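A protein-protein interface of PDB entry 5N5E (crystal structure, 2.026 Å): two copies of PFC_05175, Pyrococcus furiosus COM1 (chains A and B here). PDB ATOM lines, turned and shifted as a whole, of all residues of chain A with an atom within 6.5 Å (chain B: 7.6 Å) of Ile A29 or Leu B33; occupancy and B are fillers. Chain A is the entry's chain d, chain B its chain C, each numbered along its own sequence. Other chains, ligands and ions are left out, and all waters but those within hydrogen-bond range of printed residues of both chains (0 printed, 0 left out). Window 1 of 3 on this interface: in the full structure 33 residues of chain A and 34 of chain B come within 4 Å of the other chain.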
ATOM      1  N   ILE A  24     -13.282 -33.599 -19.029  1.00  0.00           N
ATOM      2  CA  ILE A  24     -12.140 -33.321 -18.160  1.00  0.00           C
ATOM      3  C   ILE A  24     -10.848 -33.282 -18.969  1.00  0.00           C
ATOM      4  O   ILE A  24      -9.892 -32.598 -18.587  1.00  0.00           O
ATOM      5  CB  ILE A  24     -12.054 -34.335 -17.000  1.00  0.00           C
ATOM      6  CG1 ILE A  24     -11.813 -35.755 -17.511  1.00  0.00           C
ATOM      7  CG2 ILE A  24     -13.314 -34.291 -16.157  1.00  0.00           C
ATOM      8  CD1 ILE A  24     -10.374 -36.205 -17.413  1.00  0.00           C
ATOM      9  N   LEU A  25     -10.791 -33.997 -20.095  1.00  0.00           N
ATOM     10  CA  LEU A  25      -9.628 -33.889 -20.972  1.00  0.00           C
ATOM     11  C   LEU A  25      -9.559 -32.514 -21.627  1.00  0.00           C
ATOM     12  O   LEU A  25      -8.474 -31.934 -21.748  1.00  0.00           O
ATOM     13  CB  LEU A  25      -9.656 -34.989 -22.031  1.00  0.00           C
ATOM     14  CG  LEU A  25      -9.340 -36.406 -21.544  1.00  0.00           C
ATOM     15  CD1 LEU A  25      -9.580 -37.413 -22.659  1.00  0.00           C
ATOM     16  CD2 LEU A  25      -7.903 -36.504 -21.033  1.00  0.00           C
ATOM     17  N   ARG A  26     -10.702 -31.975 -22.058  1.00  0.00           N
ATOM     18  CA  ARG A  26     -10.711 -30.613 -22.583  1.00  0.00           C
ATOM     19  C   ARG A  26     -10.333 -29.617 -21.495  1.00  0.00           C
ATOM     20  O   ARG A  26      -9.627 -28.636 -21.756  1.00  0.00           O
ATOM     21  CB  ARG A  26     -12.082 -30.280 -23.174  1.00  0.00           C
ATOM     22  CG  ARG A  26     -12.496 -31.195 -24.317  1.00  0.00           C
ATOM     23  CD  ARG A  26     -13.676 -30.645 -25.108  1.00  0.00           C
ATOM     24  NE  ARG A  26     -14.267 -31.674 -25.962  1.00  0.00           N
ATOM     25  CZ  ARG A  26     -15.289 -32.452 -25.617  1.00  0.00           C
ATOM     26  NH1 ARG A  26     -15.744 -33.360 -26.467  1.00  0.00           N
ATOM     27  NH2 ARG A  26     -15.862 -32.330 -24.424  1.00  0.00           N
ATOM     28  N   LEU A  27     -10.788 -29.859 -20.263  1.00  0.00           N
ATOM     29  CA  LEU A  27     -10.436 -28.982 -19.154  1.00  0.00           C
ATOM     30  C   LEU A  27      -8.953 -29.089 -18.821  1.00  0.00           C
ATOM     31  O   LEU A  27      -8.315 -28.088 -18.478  1.00  0.00           O
ATOM     32  CB  LEU A  27     -11.289 -29.325 -17.932  1.00  0.00           C
ATOM     33  CG  LEU A  27     -11.137 -28.428 -16.702  1.00  0.00           C
ATOM     34  CD1 LEU A  27     -11.516 -26.980 -17.018  1.00  0.00           C
ATOM     35  CD2 LEU A  27     -11.975 -28.962 -15.551  1.00  0.00           C
ATOM     36  N   ALA A  28      -8.384 -30.291 -18.929  1.00  0.00           N
ATOM     37  CA  ALA A  28      -6.947 -30.444 -18.719  1.00  0.00           C
ATOM     38  C   ALA A  28      -6.160 -29.654 -19.755  1.00  0.00           C
ATOM     39  O   ALA A  28      -5.162 -29.004 -19.426  1.00  0.00           O
ATOM     40  CB  ALA A  28      -6.564 -31.923 -18.769  1.00  0.00           C
ATOM     41  N   ILE A  29      -6.609 -29.678 -21.013  1.00  0.00           N
ATOM     42  CA  ILE A  29      -5.948 -28.891 -22.050  1.00  0.00           C
ATOM     43  C   ILE A  29      -6.062 -27.407 -21.736  1.00  0.00           C
ATOM     44  O   ILE A  29      -5.108 -26.644 -21.929  1.00  0.00           O
ATOM     45  CB  ILE A  29      -6.536 -29.227 -23.433  1.00  0.00           C
ATOM     46  CG1 ILE A  29      -6.203 -30.675 -23.803  1.00  0.00           C
ATOM     47  CG2 ILE A  29      -6.010 -28.263 -24.495  1.00  0.00           C
ATOM     48  CD1 ILE A  29      -6.959 -31.193 -25.003  1.00  0.00           C
ATOM     49  N   ILE A  30      -7.231 -26.973 -21.259  1.00  0.00           N
ATOM     50  CA  ILE A  30      -7.399 -25.584 -20.841  1.00  0.00           C
ATOM     51  C   ILE A  30      -6.362 -25.225 -19.784  1.00  0.00           C
ATOM     52  O   ILE A  30      -5.719 -24.171 -19.853  1.00  0.00           O
ATOM     53  CB  ILE A  30      -8.836 -25.347 -20.340  1.00  0.00           C
ATOM     54  CG1 ILE A  30      -9.807 -25.368 -21.522  1.00  0.00           C
ATOM     55  CG2 ILE A  30      -8.939 -24.027 -19.570  1.00  0.00           C
ATOM     56  CD1 ILE A  30     -11.273 -25.372 -21.129  1.00  0.00           C
ATOM     57  N   ALA A  31      -6.185 -26.098 -18.790  1.00  0.00           N
ATOM     58  CA  ALA A  31      -5.231 -25.825 -17.720  1.00  0.00           C
ATOM     59  C   ALA A  31      -3.811 -25.703 -18.259  1.00  0.00           C
ATOM     60  O   ALA A  31      -3.050 -24.826 -17.833  1.00  0.00           O
ATOM     61  CB  ALA A  31      -5.304 -26.925 -16.662  1.00  0.00           C
ATOM     62  N   GLU A  32      -3.433 -26.579 -19.192  1.00  0.00           N
ATOM     63  CA  GLU A  32      -2.088 -26.532 -19.757  1.00  0.00           C
ATOM     64  C   GLU A  32      -1.883 -25.275 -20.591  1.00  0.00           C
ATOM     65  O   GLU A  32      -0.839 -24.620 -20.490  1.00  0.00           O
ATOM     66  CB  GLU A  32      -1.830 -27.780 -20.602  1.00  0.00           C
ATOM     67  CG  GLU A  32      -1.795 -29.070 -19.801  1.00  0.00           C
ATOM     68  CD  GLU A  32      -0.586 -29.164 -18.889  1.00  0.00           C
ATOM     69  OE1 GLU A  32       0.414 -28.459 -19.145  1.00  0.00           O
ATOM     70  OE2 GLU A  32      -0.635 -29.943 -17.914  1.00  0.00           O
ATOM     71  N   LEU A  33      -2.862 -24.927 -21.428  1.00  0.00           N
ATOM     72  CA  LEU A  33      -2.742 -23.723 -22.243  1.00  0.00           C
ATOM     73  C   LEU A  33      -2.647 -22.480 -21.369  1.00  0.00           C
ATOM     74  O   LEU A  33      -1.906 -21.542 -21.689  1.00  0.00           O
ATOM     75  CB  LEU A  33      -3.927 -23.621 -23.202  1.00  0.00           C
ATOM     76  CG  LEU A  33      -3.991 -24.708 -24.280  1.00  0.00           C
ATOM     77  CD1 LEU A  33      -5.315 -24.655 -25.025  1.00  0.00           C
ATOM     78  CD2 LEU A  33      -2.834 -24.573 -25.255  1.00  0.00           C
ATOM     79  N   ASP A  34      -3.400 -22.448 -20.267  1.00  0.00           N
ATOM     80  CA  ASP A  34      -3.303 -21.330 -19.335  1.00  0.00           C
ATOM     81  C   ASP A  34      -1.918 -21.267 -18.698  1.00  0.00           C
ATOM     82  O   ASP A  34      -1.356 -20.181 -18.523  1.00  0.00           O
ATOM     83  CB  ASP A  34      -4.388 -21.445 -18.264  1.00  0.00           C
ATOM     84  CG  ASP A  34      -4.358 -20.294 -17.274  1.00  0.00           C
ATOM     85  OD1 ASP A  34      -4.366 -19.129 -17.717  1.00  0.00           O
ATOM     86  OD2 ASP A  34      -4.338 -20.556 -16.052  1.00  0.00           O
ATOM     87  N   HIS A  65       2.507 -31.715 -22.534  1.00  0.00           N
ATOM     88  CA  HIS A  65       1.300 -32.153 -21.842  1.00  0.00           C
ATOM     89  C   HIS A  65       0.060 -31.901 -22.691  1.00  0.00           C
ATOM     90  O   HIS A  65      -0.881 -32.704 -22.679  1.00  0.00           O
ATOM     91  CB  HIS A  65       1.183 -31.448 -20.492  1.00  0.00           C
ATOM     92  CG  HIS A  65       2.264 -31.817 -19.526  1.00  0.00           C
ATOM     93  ND1 HIS A  65       2.520 -31.094 -18.381  1.00  0.00           N
ATOM     94  CD2 HIS A  65       3.154 -32.838 -19.532  1.00  0.00           C
ATOM     95  CE1 HIS A  65       3.522 -31.651 -17.725  1.00  0.00           C
ATOM     96  NE2 HIS A  65       3.925 -32.711 -18.402  1.00  0.00           N
ATOM     97  N   VAL A  66       0.029 -30.784 -23.422  1.00  0.00           N
ATOM     98  CA  VAL A  66      -1.067 -30.546 -24.358  1.00  0.00           C
ATOM     99  C   VAL A  66      -1.184 -31.712 -25.329  1.00  0.00           C
ATOM    100  O   VAL A  66      -2.285 -32.206 -25.605  1.00  0.00           O
ATOM    101  CB  VAL A  66      -0.862 -29.215 -25.105  1.00  0.00           C
ATOM    102  CG1 VAL A  66      -1.903 -29.050 -26.214  1.00  0.00           C
ATOM    103  CG2 VAL A  66      -0.914 -28.038 -24.140  1.00  0.00           C
ATOM    104  N   PHE A  69      -2.696 -34.952 -23.493  1.00  0.00           N
ATOM    105  CA  PHE A  69      -4.141 -34.870 -23.308  1.00  0.00           C
ATOM    106  C   PHE A  69      -4.864 -34.856 -24.648  1.00  0.00           C
ATOM    107  O   PHE A  69      -5.935 -35.459 -24.788  1.00  0.00           O
ATOM    108  CB  PHE A  69      -4.495 -33.628 -22.489  1.00  0.00           C
ATOM    109  CG  PHE A  69      -4.037 -33.690 -21.057  1.00  0.00           C
ATOM    110  CD1 PHE A  69      -4.299 -34.805 -20.274  1.00  0.00           C
ATOM    111  CD2 PHE A  69      -3.348 -32.631 -20.493  1.00  0.00           C
ATOM    112  CE1 PHE A  69      -3.880 -34.860 -18.955  1.00  0.00           C
ATOM    113  CE2 PHE A  69      -2.924 -32.681 -19.176  1.00  0.00           C
ATOM    114  CZ  PHE A  69      -3.194 -33.796 -18.407  1.00  0.00           C
ATOM    115  N   MET A  70      -4.293 -34.183 -25.650  1.00  0.00           N
ATOM    116  CA  MET A  70      -4.904 -34.167 -26.973  1.00  0.00           C
ATOM    117  C   MET A  70      -4.999 -35.575 -27.553  1.00  0.00           C
ATOM    118  O   MET A  70      -6.029 -35.951 -28.125  1.00  0.00           O
ATOM    119  CB  MET A  70      -4.104 -33.257 -27.906  1.00  0.00           C
ATOM    120  CG  MET A  70      -4.731 -33.058 -29.279  1.00  0.00           C
ATOM    121  SD  MET A  70      -6.241 -32.075 -29.227  1.00  0.00           S
ATOM    122  CE  MET A  70      -5.562 -30.450 -28.898  1.00  0.00           C
ATOM    123  N   ALA A  71      -3.933 -36.370 -27.415  1.00  0.00           N
ATOM    124  CA  ALA A  71      -3.957 -37.735 -27.934  1.00  0.00           C
ATOM    125  C   ALA A  71      -5.091 -38.537 -27.311  1.00  0.00           C
ATOM    126  O   ALA A  71      -5.797 -39.273 -28.010  1.00  0.00           O
ATOM    127  CB  ALA A  71      -2.616 -38.423 -27.681  1.00  0.00           C
ATOM    128  N   LEU A  73      -7.841 -37.237 -25.951  1.00  0.00           N
ATOM    129  CA  LEU A  73      -9.101 -36.639 -26.381  1.00  0.00           C
ATOM    130  C   LEU A  73      -9.476 -37.116 -27.776  1.00  0.00           C
ATOM    131  O   LEU A  73     -10.619 -37.512 -28.026  1.00  0.00           O
ATOM    132  CB  LEU A  73      -8.996 -35.113 -26.349  1.00  0.00           C
ATOM    133  CG  LEU A  73     -10.211 -34.341 -26.882  1.00  0.00           C
ATOM    134  CD1 LEU A  73     -11.447 -34.622 -26.040  1.00  0.00           C
ATOM    135  CD2 LEU A  73      -9.916 -32.851 -26.943  1.00  0.00           C
ATOM    136  N   GLN A  80     -13.842 -34.966 -32.968  1.00  0.00           N
ATOM    137  CA  GLN A  80     -12.771 -33.975 -32.907  1.00  0.00           C
ATOM    138  C   GLN A  80     -11.681 -34.268 -33.929  1.00  0.00           C
ATOM    139  O   GLN A  80     -11.079 -33.337 -34.476  1.00  0.00           O
ATOM    140  CB  GLN A  80     -12.180 -33.933 -31.497  1.00  0.00           C
ATOM    141  CG  GLN A  80     -11.101 -32.875 -31.277  1.00  0.00           C
ATOM    142  CD  GLN A  80     -11.607 -31.459 -31.479  1.00  0.00           C
ATOM    143  OE1 GLN A  80     -12.255 -30.890 -30.601  1.00  0.00           O
ATOM    144  NE2 GLN A  80     -11.285 -30.870 -32.625  1.00  0.00           N
ATOM    145  N   ARG B  26      -3.921 -19.397 -27.995  1.00  0.00           N
ATOM    146  CA  ARG B  26      -4.179 -20.361 -26.929  1.00  0.00           C
ATOM    147  C   ARG B  26      -5.449 -20.002 -26.169  1.00  0.00           C
ATOM    148  O   ARG B  26      -6.228 -20.886 -25.791  1.00  0.00           O
ATOM    149  CB  ARG B  26      -2.984 -20.429 -25.976  1.00  0.00           C
ATOM    150  CG  ARG B  26      -1.683 -20.837 -26.652  1.00  0.00           C
ATOM    151  CD  ARG B  26      -0.608 -21.225 -25.648  1.00  0.00           C
ATOM    152  NE  ARG B  26       0.716 -21.290 -26.268  1.00  0.00           N
ATOM    153  CZ  ARG B  26       1.594 -20.290 -26.299  1.00  0.00           C
ATOM    154  NH1 ARG B  26       2.765 -20.461 -26.895  1.00  0.00           N
ATOM    155  NH2 ARG B  26       1.314 -19.121 -25.741  1.00  0.00           N
ATOM    156  N   LEU B  27      -5.681 -18.707 -25.942  1.00  0.00           N
ATOM    157  CA  LEU B  27      -6.896 -18.284 -25.256  1.00  0.00           C
ATOM    158  C   LEU B  27      -8.128 -18.549 -26.112  1.00  0.00           C
ATOM    159  O   LEU B  27      -9.186 -18.917 -25.589  1.00  0.00           O
ATOM    160  CB  LEU B  27      -6.797 -16.800 -24.897  1.00  0.00           C
ATOM    161  CG  LEU B  27      -7.938 -16.208 -24.066  1.00  0.00           C
ATOM    162  CD1 LEU B  27      -8.062 -16.911 -22.722  1.00  0.00           C
ATOM    163  CD2 LEU B  27      -7.734 -14.717 -23.866  1.00  0.00           C
ATOM    164  N   ALA B  28      -8.009 -18.382 -27.431  1.00  0.00           N
ATOM    165  CA  ALA B  28      -9.120 -18.712 -28.318  1.00  0.00           C
ATOM    166  C   ALA B  28      -9.454 -20.196 -28.251  1.00  0.00           C
ATOM    167  O   ALA B  28     -10.630 -20.577 -28.269  1.00  0.00           O
ATOM    168  CB  ALA B  28      -8.787 -18.296 -29.751  1.00  0.00           C
ATOM    169  N   ILE B  29      -8.431 -21.052 -28.186  1.00  0.00           N
ATOM    170  CA  ILE B  29      -8.658 -22.488 -28.040  1.00  0.00           C
ATOM    171  C   ILE B  29      -9.321 -22.787 -26.701  1.00  0.00           C
ATOM    172  O   ILE B  29     -10.230 -23.624 -26.612  1.00  0.00           O
ATOM    173  CB  ILE B  29      -7.330 -23.253 -28.206  1.00  0.00           C
ATOM    174  CG1 ILE B  29      -6.805 -23.093 -29.635  1.00  0.00           C
ATOM    175  CG2 ILE B  29      -7.506 -24.729 -27.870  1.00  0.00           C
ATOM    176  CD1 ILE B  29      -5.374 -23.560 -29.826  1.00  0.00           C
ATOM    177  N   ILE B  30      -8.873 -22.116 -25.639  1.00  0.00           N
ATOM    178  CA  ILE B  30      -9.508 -22.267 -24.331  1.00  0.00           C
ATOM    179  C   ILE B  30     -10.995 -21.948 -24.429  1.00  0.00           C
ATOM    180  O   ILE B  30     -11.843 -22.672 -23.894  1.00  0.00           O
ATOM    181  CB  ILE B  30      -8.804 -21.372 -23.294  1.00  0.00           C
ATOM    182  CG1 ILE B  30      -7.420 -21.937 -22.966  1.00  0.00           C
ATOM    183  CG2 ILE B  30      -9.657 -21.222 -22.020  1.00  0.00           C
ATOM    184  CD1 ILE B  30      -6.549 -21.014 -22.134  1.00  0.00           C
ATOM    185  N   ALA B  31     -11.330 -20.844 -25.101  1.00  0.00           N
ATOM    186  CA  ALA B  31     -12.729 -20.446 -25.227  1.00  0.00           C
ATOM    187  C   ALA B  31     -13.534 -21.494 -25.987  1.00  0.00           C
ATOM    188  O   ALA B  31     -14.671 -21.806 -25.614  1.00  0.00           O
ATOM    189  CB  ALA B  31     -12.823 -19.089 -25.923  1.00  0.00           C
ATOM    190  N   GLU B  32     -12.958 -22.047 -27.055  1.00  0.00           N
ATOM    191  CA  GLU B  32     -13.657 -23.062 -27.836  1.00  0.00           C
ATOM    192  C   GLU B  32     -13.857 -24.339 -27.029  1.00  0.00           C
ATOM    193  O   GLU B  32     -14.941 -24.932 -27.056  1.00  0.00           O
ATOM    194  CB  GLU B  32     -12.881 -23.354 -29.121  1.00  0.00           C
ATOM    195  CG  GLU B  32     -12.841 -22.187 -30.100  1.00  0.00           C
ATOM    196  CD  GLU B  32     -14.195 -21.903 -30.723  1.00  0.00           C
ATOM    197  OE1 GLU B  32     -15.049 -22.813 -30.725  1.00  0.00           O
ATOM    198  OE2 GLU B  32     -14.407 -20.772 -31.210  1.00  0.00           O
ATOM    199  N   LEU B  33     -12.820 -24.786 -26.317  1.00  0.00           N
ATOM    200  CA  LEU B  33     -12.949 -25.986 -25.499  1.00  0.00           C
ATOM    201  C   LEU B  33     -13.993 -25.794 -24.407  1.00  0.00           C
ATOM    202  O   LEU B  33     -14.738 -26.725 -24.079  1.00  0.00           O
ATOM    203  CB  LEU B  33     -11.595 -26.355 -24.892  1.00  0.00           C
ATOM    204  CG  LEU B  33     -10.522 -26.805 -25.889  1.00  0.00           C
ATOM    205  CD1 LEU B  33      -9.169 -26.906 -25.211  1.00  0.00           C
ATOM    206  CD2 LEU B  33     -10.897 -28.139 -26.515  1.00  0.00           C
ATOM    207  N   ASP B  34     -14.055 -24.595 -23.822  1.00  0.00           N
ATOM    208  CA  ASP B  34     -15.084 -24.316 -22.827  1.00  0.00           C
ATOM    209  C   ASP B  34     -16.474 -24.381 -23.449  1.00  0.00           C
ATOM    210  O   ASP B  34     -17.409 -24.915 -22.843  1.00  0.00           O
ATOM    211  CB  ASP B  34     -14.845 -22.948 -22.188  1.00  0.00           C
ATOM    212  CG  ASP B  34     -15.870 -22.616 -21.115  1.00  0.00           C
ATOM    213  OD1 ASP B  34     -16.062 -23.441 -20.196  1.00  0.00           O
ATOM    214  OD2 ASP B  34     -16.486 -21.531 -21.189  1.00  0.00           O
ATOM    215  N   ALA B  35     -16.626 -23.843 -24.663  1.00  0.00           N
ATOM    216  CA  ALA B  35     -17.921 -23.872 -25.337  1.00  0.00           C
ATOM    217  C   ALA B  35     -18.345 -25.299 -25.663  1.00  0.00           C
ATOM    218  O   ALA B  35     -19.525 -25.647 -25.534  1.00  0.00           O
ATOM    219  CB  ALA B  35     -17.868 -23.029 -26.611  1.00  0.00           C
ATOM    220  N   ILE B  36     -17.406 -26.135 -26.107  1.00  0.00           N
ATOM    221  CA  ILE B  36     -17.728 -27.532 -26.384  1.00  0.00           C
ATOM    222  C   ILE B  36     -18.235 -28.213 -25.118  1.00  0.00           C
ATOM    223  O   ILE B  36     -19.281 -28.873 -25.122  1.00  0.00           O
ATOM    224  CB  ILE B  36     -16.507 -28.261 -26.976  1.00  0.00           C
ATOM    225  CG1 ILE B  36     -16.139 -27.657 -28.333  1.00  0.00           C
ATOM    226  CG2 ILE B  36     -16.796 -29.751 -27.150  1.00  0.00           C
ATOM    227  CD1 ILE B  36     -14.757 -28.038 -28.828  1.00  0.00           C
ATOM    228  N   ASN B  37     -17.498 -28.064 -24.014  1.00  0.00           N
ATOM    229  CA  ASN B  37     -17.942 -28.652 -22.752  1.00  0.00           C
ATOM    230  C   ASN B  37     -19.323 -28.139 -22.364  1.00  0.00           C
ATOM    231  O   ASN B  37     -20.165 -28.904 -21.878  1.00  0.00           O
ATOM    232  CB  ASN B  37     -16.935 -28.355 -21.641  1.00  0.00           C
ATOM    233  CG  ASN B  37     -15.771 -29.334 -21.624  1.00  0.00           C
ATOM    234  OD1 ASN B  37     -15.601 -30.136 -22.541  1.00  0.00           O
ATOM    235  ND2 ASN B  37     -14.973 -29.282 -20.564  1.00  0.00           N
ATOM    236  N   LEU B  38     -19.567 -26.841 -22.549  1.00  0.00           N
ATOM    237  CA  LEU B  38     -20.864 -26.274 -22.198  1.00  0.00           C
ATOM    238  C   LEU B  38     -21.976 -26.912 -23.020  1.00  0.00           C
ATOM    239  O   LEU B  38     -22.992 -27.358 -22.474  1.00  0.00           O
ATOM    240  CB  LEU B  38     -20.845 -24.760 -22.404  1.00  0.00           C
ATOM    241  CG  LEU B  38     -22.141 -24.030 -22.040  1.00  0.00           C
ATOM    242  CD1 LEU B  38     -22.390 -24.082 -20.536  1.00  0.00           C
ATOM    243  CD2 LEU B  38     -22.093 -22.597 -22.539  1.00  0.00           C
ATOM    244  N   TYR B  39     -21.800 -26.964 -24.343  1.00  0.00           N
ATOM    245  CA  TYR B  39     -22.853 -27.478 -25.212  1.00  0.00           C
ATOM    246  C   TYR B  39     -23.004 -28.987 -25.082  1.00  0.00           C
ATOM    247  O   TYR B  39     -24.119 -29.509 -25.209  1.00  0.00           O
ATOM    248  CB  TYR B  39     -22.565 -27.084 -26.662  1.00  0.00           C
ATOM    249  CG  TYR B  39     -22.510 -25.583 -26.885  1.00  0.00           C
ATOM    250  CD1 TYR B  39     -23.237 -24.712 -26.079  1.00  0.00           C
ATOM    251  CD2 TYR B  39     -21.728 -25.039 -27.894  1.00  0.00           C
ATOM    252  CE1 TYR B  39     -23.189 -23.345 -26.278  1.00  0.00           C
ATOM    253  CE2 TYR B  39     -21.673 -23.673 -28.098  1.00  0.00           C
ATOM    254  CZ  TYR B  39     -22.405 -22.832 -27.288  1.00  0.00           C
ATOM    255  OH  TYR B  39     -22.355 -21.472 -27.489  1.00  0.00           O
ATOM    256  N   GLU B  62     -17.731 -25.999 -33.256  1.00  0.00           N
ATOM    257  CA  GLU B  62     -16.702 -25.457 -32.375  1.00  0.00           C
ATOM    258  C   GLU B  62     -15.445 -26.317 -32.408  1.00  0.00           C
ATOM    259  O   GLU B  62     -14.331 -25.796 -32.282  1.00  0.00           O
ATOM    260  CB  GLU B  62     -17.214 -25.351 -30.934  1.00  0.00           C
ATOM    261  CG  GLU B  62     -18.582 -24.691 -30.759  1.00  0.00           C
ATOM    262  CD  GLU B  62     -18.625 -23.231 -31.185  1.00  0.00           C
ATOM    263  OE1 GLU B  62     -17.659 -22.746 -31.808  1.00  0.00           O
ATOM    264  OE2 GLU B  62     -19.645 -22.567 -30.899  1.00  0.00           O
ATOM    265  N   LYS B  63     -15.602 -27.631 -32.579  1.00  0.00           N
ATOM    266  CA  LYS B  63     -14.438 -28.505 -32.683  1.00  0.00           C
ATOM    267  C   LYS B  63     -13.612 -28.179 -33.920  1.00  0.00           C
ATOM    268  O   LYS B  63     -12.384 -28.322 -33.902  1.00  0.00           O
ATOM    269  CB  LYS B  63     -14.886 -29.967 -32.701  1.00  0.00           C
ATOM    270  CG  LYS B  63     -15.496 -30.425 -31.386  1.00  0.00           C
ATOM    271  CD  LYS B  63     -16.045 -31.841 -31.471  1.00  0.00           C
ATOM    272  CE  LYS B  63     -16.733 -32.236 -30.173  1.00  0.00           C
ATOM    273  NZ  LYS B  63     -17.262 -33.619 -30.203  1.00  0.00           N
ATOM    274  N   VAL B  66     -11.490 -25.208 -33.027  1.00  0.00           N
ATOM    275  CA  VAL B  66     -10.275 -25.662 -32.355  1.00  0.00           C
ATOM    276  C   VAL B  66      -9.196 -25.980 -33.381  1.00  0.00           C
ATOM    277  O   VAL B  66      -8.028 -25.609 -33.215  1.00  0.00           O
ATOM    278  CB  VAL B  66     -10.580 -26.878 -31.458  1.00  0.00           C
ATOM    279  CG1 VAL B  66      -9.294 -27.481 -30.899  1.00  0.00           C
ATOM    280  CG2 VAL B  66     -11.508 -26.482 -30.327  1.00  0.00           C
ATOM    281  N   MET B  70      -5.744 -24.022 -33.739  1.00  0.00           N
ATOM    282  CA  MET B  70      -4.566 -24.865 -33.551  1.00  0.00           C
ATOM    283  C   MET B  70      -3.635 -24.781 -34.754  1.00  0.00           C
ATOM    284  O   MET B  70      -2.408 -24.744 -34.597  1.00  0.00           O
ATOM    285  CB  MET B  70      -4.994 -26.311 -33.301  1.00  0.00           C
ATOM    286  CG  MET B  70      -3.842 -27.302 -33.219  1.00  0.00           C
ATOM    287  SD  MET B  70      -3.897 -28.300 -31.722  1.00  0.00           S
ATOM    288  CE  MET B  70      -3.586 -27.042 -30.488  1.00  0.00           C
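Among the printed residues, pairs that only touch across the chains: Arg A26 with Leu B33, Arg A26 with Ile B36, Arg A26 with Lys B63, Ile A29 with Leu B33, Ile A30 with Ile B30, Ile A30 with Leu B33, Ile A30 with Asp B34, Leu A33 with Arg B26, Leu A33 with Ile B29, Leu A33 with Ile B30, Asp A34 with Ile B30 and Met A70 with Met B70.
Arg A26 touches Leu B33, and with the chains exchanged Leu A33 touches Arg B26. Ile A29 touches Leu B33, and with the chains exchanged Leu A33 touches Ile B29. Ile A30 touches Asp B34, and with the chains exchanged Asp A34 touches Ile B30. Met B70 touches its own counterpart, Met A70. Positions printed for both chains: 26, 27, 28, 29, 30, 31, 32, 33, 34, 66 and 70. Of the 14 pairs that touch across the chains among the printed residues, 10 have their exchanged pair printed and touching as well.
Leu B33 touches just these residues of chain A: Arg A26, Ile A29 and Ile A30. No residue of chain B comes within 4 Å of Ala A28. Of the printed residues of chain A, Asp B34 touches Ile A30. Of the printed residues of chain B, Asp A34 touches Ile B30. Printed residues of chain B within 4 Å of Arg A26: Leu B33 (3.9 Å), Ile B36 (3.4 Å), Asn B37 (2.9 Å) and Lys B63 (3.997 Å). Printed residues of chain B within 4 Å of Leu A33: Arg B26, Ile B29 and Ile B30. The nearest residue of chain A that does not touch Leu B33 is Leu A33 (4.5 Å). The nearest printed residue of chain B that does not touch Asp A34 is Arg B26 (6.1 Å).
The backbone carbonyl oxygen (O) of Lys B63 sits at hydrogen-bond distance from the side-chain amide nitrogen (NE2) of Gln A80 (3.1 Å). NH2 of Arg A26 lies within hydrogen-bond range of OD1 of Asn B37.
Printed residues of chain A that touch a printed residue of chain B: Arg A26, Ile A29, Ile A30, Leu A33, Asp A34, Met A70 and Gln A80. Among the printed residues, no Asp or Glu carboxylate lies within 4 Å of a Lys or Arg side-chain nitrogen of the other chain.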
